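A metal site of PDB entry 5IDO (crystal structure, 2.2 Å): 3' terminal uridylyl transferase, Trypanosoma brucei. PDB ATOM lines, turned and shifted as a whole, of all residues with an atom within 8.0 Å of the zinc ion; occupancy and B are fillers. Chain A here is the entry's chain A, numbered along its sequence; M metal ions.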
ATOM      1  N   SER A   7      -3.960  -3.734 -29.926  1.00  0.00           N
ATOM      2  CA  SER A   7      -2.898  -3.798 -28.926  1.00  0.00           C
ATOM      3  C   SER A   7      -2.515  -5.243 -28.595  1.00  0.00           C
ATOM      4  O   SER A   7      -3.352  -6.144 -28.613  1.00  0.00           O
ATOM      5  CB  SER A   7      -3.305  -3.053 -27.660  1.00  0.00           C
ATOM      6  OG  SER A   7      -4.385  -3.689 -26.999  1.00  0.00           O
ATOM      7  N   CYS A   8      -1.234  -5.438 -28.297  1.00  0.00           N
ATOM      8  CA  CYS A   8      -0.736  -6.757 -27.927  1.00  0.00           C
ATOM      9  C   CYS A   8      -1.023  -7.069 -26.468  1.00  0.00           C
ATOM     10  O   CYS A   8      -1.283  -6.162 -25.676  1.00  0.00           O
ATOM     11  CB  CYS A   8       0.762  -6.851 -28.200  1.00  0.00           C
ATOM     12  SG  CYS A   8       1.478  -8.466 -27.816  1.00  0.00           S
ATOM     13  N   ASP A   9      -0.975  -8.345 -26.098  1.00  0.00           N
ATOM     14  CA  ASP A   9      -1.204  -8.744 -24.722  1.00  0.00           C
ATOM     15  C   ASP A   9       0.071  -9.305 -24.083  1.00  0.00           C
ATOM     16  O   ASP A   9       0.065  -9.712 -22.921  1.00  0.00           O
ATOM     17  CB  ASP A   9      -2.328  -9.791 -24.640  1.00  0.00           C
ATOM     18  CG  ASP A   9      -1.950 -11.098 -25.314  1.00  0.00           C
ATOM     19  OD1 ASP A   9      -1.217 -11.056 -26.331  1.00  0.00           O
ATOM     20  OD2 ASP A   9      -2.396 -12.159 -24.829  1.00  0.00           O
ATOM     21  N   ALA A  10       1.151  -9.295 -24.850  1.00  0.00           N
ATOM     22  CA  ALA A  10       2.428  -9.861 -24.395  1.00  0.00           C
ATOM     23  C   ALA A  10       3.391  -8.763 -23.957  1.00  0.00           C
ATOM     24  O   ALA A  10       4.429  -9.050 -23.342  1.00  0.00           O
ATOM     25  CB  ALA A  10       3.042 -10.703 -25.497  1.00  0.00           C
ATOM     26  N   CYS A  11       3.059  -7.529 -24.280  1.00  0.00           N
ATOM     27  CA  CYS A  11       3.826  -6.366 -23.853  1.00  0.00           C
ATOM     28  C   CYS A  11       2.940  -5.126 -23.908  1.00  0.00           C
ATOM     29  O   CYS A  11       2.066  -5.033 -24.776  1.00  0.00           O
ATOM     30  CB  CYS A  11       5.076  -6.189 -24.715  1.00  0.00           C
ATOM     31  SG  CYS A  11       4.798  -5.310 -26.255  1.00  0.00           S
ATOM     32  N   PRO A  12       3.156  -4.170 -22.996  1.00  0.00           N
ATOM     33  CA  PRO A  12       2.243  -3.025 -22.866  1.00  0.00           C
ATOM     34  C   PRO A  12       2.455  -1.926 -23.908  1.00  0.00           C
ATOM     35  O   PRO A  12       1.650  -0.997 -23.973  1.00  0.00           O
ATOM     36  CB  PRO A  12       2.557  -2.500 -21.465  1.00  0.00           C
ATOM     37  CG  PRO A  12       4.010  -2.810 -21.287  1.00  0.00           C
ATOM     38  CD  PRO A  12       4.242  -4.114 -22.008  1.00  0.00           C
ATOM     39  N   HIS A  13       3.511  -2.032 -24.712  1.00  0.00           N
ATOM     40  CA  HIS A  13       3.842  -0.967 -25.655  1.00  0.00           C
ATOM     41  C   HIS A  13       3.878  -1.434 -27.113  1.00  0.00           C
ATOM     42  O   HIS A  13       4.915  -1.383 -27.771  1.00  0.00           O
ATOM     43  CB  HIS A  13       5.193  -0.351 -25.282  1.00  0.00           C
ATOM     44  CG  HIS A  13       6.246  -1.357 -24.923  1.00  0.00           C
ATOM     45  ND1 HIS A  13       6.666  -1.565 -23.630  1.00  0.00           N
ATOM     46  CD2 HIS A  13       6.959  -2.209 -25.695  1.00  0.00           C
ATOM     47  CE1 HIS A  13       7.591  -2.504 -23.614  1.00  0.00           C
ATOM     48  NE2 HIS A  13       7.781  -2.915 -24.856  1.00  0.00           N
ATOM     49  N   ALA A  14       2.736  -1.893 -27.614  1.00  0.00           N
ATOM     50  CA  ALA A  14       2.631  -2.343 -28.998  1.00  0.00           C
ATOM     51  C   ALA A  14       1.214  -2.179 -29.527  1.00  0.00           C
ATOM     52  O   ALA A  14       0.289  -2.835 -29.052  1.00  0.00           O
ATOM     53  CB  ALA A  14       3.087  -3.788 -29.104  1.00  0.00           C
ATOM     54  N   VAL A  15       1.051  -1.297 -30.514  1.00  0.00           N
ATOM     55  CA  VAL A  15      -0.243  -1.072 -31.133  1.00  0.00           C
ATOM     56  C   VAL A  15      -0.134  -0.945 -32.651  1.00  0.00           C
ATOM     57  O   VAL A  15       0.842  -0.410 -33.167  1.00  0.00           O
ATOM     58  CB  VAL A  15      -0.931   0.193 -30.585  1.00  0.00           C
ATOM     59  CG1 VAL A  15      -1.748  -0.137 -29.346  1.00  0.00           C
ATOM     60  CG2 VAL A  15       0.094   1.277 -30.296  1.00  0.00           C
ATOM     61  N   PHE A  16      -1.149  -1.446 -33.344  1.00  0.00           N
ATOM     62  CA  PHE A  16      -1.154  -1.439 -34.805  1.00  0.00           C
ATOM     63  C   PHE A  16      -2.496  -0.957 -35.323  1.00  0.00           C
ATOM     64  O   PHE A  16      -3.437  -0.733 -34.551  1.00  0.00           O
ATOM     65  CB  PHE A  16      -0.829  -2.838 -35.345  1.00  0.00           C
ATOM     66  CG  PHE A  16       0.411  -3.435 -34.745  1.00  0.00           C
ATOM     67  CD1 PHE A  16       0.349  -4.139 -33.560  1.00  0.00           C
ATOM     68  CD2 PHE A  16       1.631  -3.292 -35.376  1.00  0.00           C
ATOM     69  CE1 PHE A  16       1.488  -4.696 -32.998  1.00  0.00           C
ATOM     70  CE2 PHE A  16       2.776  -3.845 -34.826  1.00  0.00           C
ATOM     71  CZ  PHE A  16       2.704  -4.547 -33.636  1.00  0.00           C
ATOM     72  N   LEU A  22      -0.593  -7.196 -36.097  1.00  0.00           N
ATOM     73  CA  LEU A  22      -0.641  -7.661 -34.719  1.00  0.00           C
ATOM     74  C   LEU A  22      -0.294  -9.153 -34.640  1.00  0.00           C
ATOM     75  O   LEU A  22       0.257  -9.610 -33.651  1.00  0.00           O
ATOM     76  CB  LEU A  22      -2.007  -7.401 -34.103  1.00  0.00           C
ATOM     77  CG  LEU A  22      -2.162  -7.735 -32.616  1.00  0.00           C
ATOM     78  CD1 LEU A  22      -1.357  -6.775 -31.758  1.00  0.00           C
ATOM     79  CD2 LEU A  22      -3.630  -7.734 -32.203  1.00  0.00           C
ATOM     80  N   HIS A  25       3.544  -9.447 -35.514  1.00  0.00           N
ATOM     81  CA  HIS A  25       4.242  -9.007 -34.313  1.00  0.00           C
ATOM     82  C   HIS A  25       4.399 -10.144 -33.303  1.00  0.00           C
ATOM     83  O   HIS A  25       5.511 -10.437 -32.860  1.00  0.00           O
ATOM     84  CB  HIS A  25       3.504  -7.849 -33.670  1.00  0.00           C
ATOM     85  CG  HIS A  25       4.091  -7.404 -32.374  1.00  0.00           C
ATOM     86  ND1 HIS A  25       5.253  -6.658 -32.302  1.00  0.00           N
ATOM     87  CD2 HIS A  25       3.691  -7.600 -31.098  1.00  0.00           C
ATOM     88  CE1 HIS A  25       5.529  -6.409 -31.036  1.00  0.00           C
ATOM     89  NE2 HIS A  25       4.601  -6.975 -30.289  1.00  0.00           N
ATOM     90  N   ALA A  26       3.288 -10.775 -32.949  1.00  0.00           N
ATOM     91  CA  ALA A  26       3.310 -11.883 -31.998  1.00  0.00           C
ATOM     92  C   ALA A  26       4.164 -13.025 -32.517  1.00  0.00           C
ATOM     93  O   ALA A  26       4.896 -13.663 -31.751  1.00  0.00           O
ATOM     94  CB  ALA A  26       1.885 -12.364 -31.719  1.00  0.00           C
ATOM     95  N   HIS A  29       8.368 -11.341 -32.421  1.00  0.00           N
ATOM     96  CA  HIS A  29       9.038 -11.060 -31.158  1.00  0.00           C
ATOM     97  C   HIS A  29       8.336 -11.687 -29.958  1.00  0.00           C
ATOM     98  O   HIS A  29       8.559 -11.273 -28.811  1.00  0.00           O
ATOM     99  CB  HIS A  29       9.169  -9.543 -30.966  1.00  0.00           C
ATOM    100  CG  HIS A  29      10.424  -9.130 -30.256  1.00  0.00           C
ATOM    101  ND1 HIS A  29      11.146  -9.986 -29.464  1.00  0.00           N
ATOM    102  CD2 HIS A  29      11.096  -7.955 -30.250  1.00  0.00           C
ATOM    103  CE1 HIS A  29      12.205  -9.361 -28.979  1.00  0.00           C
ATOM    104  NE2 HIS A  29      12.198  -8.122 -29.442  1.00  0.00           N
ATOM    105  N   HIS A  30       7.506 -12.687 -30.192  1.00  0.00           N
ATOM    106  CA  HIS A  30       6.850 -13.406 -29.101  1.00  0.00           C
ATOM    107  C   HIS A  30       6.678 -14.885 -29.392  1.00  0.00           C
ATOM    108  O   HIS A  30       5.790 -15.540 -28.840  1.00  0.00           O
ATOM    109  CB  HIS A  30       5.496 -12.781 -28.790  1.00  0.00           C
ATOM    110  CG  HIS A  30       5.599 -11.470 -28.069  1.00  0.00           C
ATOM    111  ND1 HIS A  30       6.213 -11.348 -26.850  1.00  0.00           N
ATOM    112  CD2 HIS A  30       5.182 -10.228 -28.407  1.00  0.00           C
ATOM    113  CE1 HIS A  30       6.175 -10.084 -26.459  1.00  0.00           C
ATOM    114  NE2 HIS A  30       5.554  -9.386 -27.389  1.00  0.00           N
ATOM    115  N   LEU A  33       6.310 -17.416 -26.489  1.00  0.00           N
ATOM    116  CA  LEU A  33       5.026 -17.694 -25.855  1.00  0.00           C
ATOM    117  C   LEU A  33       4.243 -18.697 -26.676  1.00  0.00           C
ATOM    118  O   LEU A  33       3.399 -19.432 -26.146  1.00  0.00           O
ATOM    119  CB  LEU A  33       4.231 -16.400 -25.686  1.00  0.00           C
ATOM    120  CG  LEU A  33       4.914 -15.284 -24.902  1.00  0.00           C
ATOM    121  CD1 LEU A  33       3.969 -14.113 -24.729  1.00  0.00           C
ATOM    122  CD2 LEU A  33       5.380 -15.815 -23.550  1.00  0.00           C
ATOM    123  N   VAL A 481      -3.841 -11.856 -28.143  1.00  0.00           N
ATOM    124  CA  VAL A 481      -3.354 -12.440 -29.386  1.00  0.00           C
ATOM    125  C   VAL A 481      -2.341 -13.582 -29.190  1.00  0.00           C
ATOM    126  O   VAL A 481      -2.470 -14.630 -29.814  1.00  0.00           O
ATOM    127  CB  VAL A 481      -2.749 -11.358 -30.324  1.00  0.00           C
ATOM    128  CG1 VAL A 481      -1.767 -10.464 -29.566  1.00  0.00           C
ATOM    129  CG2 VAL A 481      -2.087 -12.000 -31.531  1.00  0.00           C
ATOM    130  N   THR A 482      -1.348 -13.377 -28.330  1.00  0.00           N
ATOM    131  CA  THR A 482      -0.383 -14.436 -28.069  1.00  0.00           C
ATOM    132  C   THR A 482      -1.076 -15.633 -27.402  1.00  0.00           C
ATOM    133  O   THR A 482      -0.828 -16.784 -27.760  1.00  0.00           O
ATOM    134  CB  THR A 482       0.795 -13.953 -27.190  1.00  0.00           C
ATOM    135  OG1 THR A 482       0.298 -13.316 -26.008  1.00  0.00           O
ATOM    136  CG2 THR A 482       1.659 -12.957 -27.975  1.00  0.00           C
HETATM  137 ZN    ZN M   1       4.061  -7.520 -27.917  1.00  0.00          ZN
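The backbone NH (N) of Cys 8 sits at hydrogen-bond distance from the backbone carbonyl oxygen (O) of Ala 14 (3.1 Å).
SG of Cys 8 lies close to N of Ala 10.
Of the 18 residues printed, 4 come within 4 Å of the zinc ion.
The nearest printed residue that does not touch the zinc ion is Ala 14 (4.04 Å).
NE2 of His 30 binds the zinc ion, 2.4 Å away.
NE2 of His 25 binds the zinc ion (2.5 Å).
SG of Cys 8 binds the zinc ion, at 2.8 Å.
Slightly farther from the zinc ion lies the side-chain sulfur (SG) of Cys 11 (2.9 Å).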
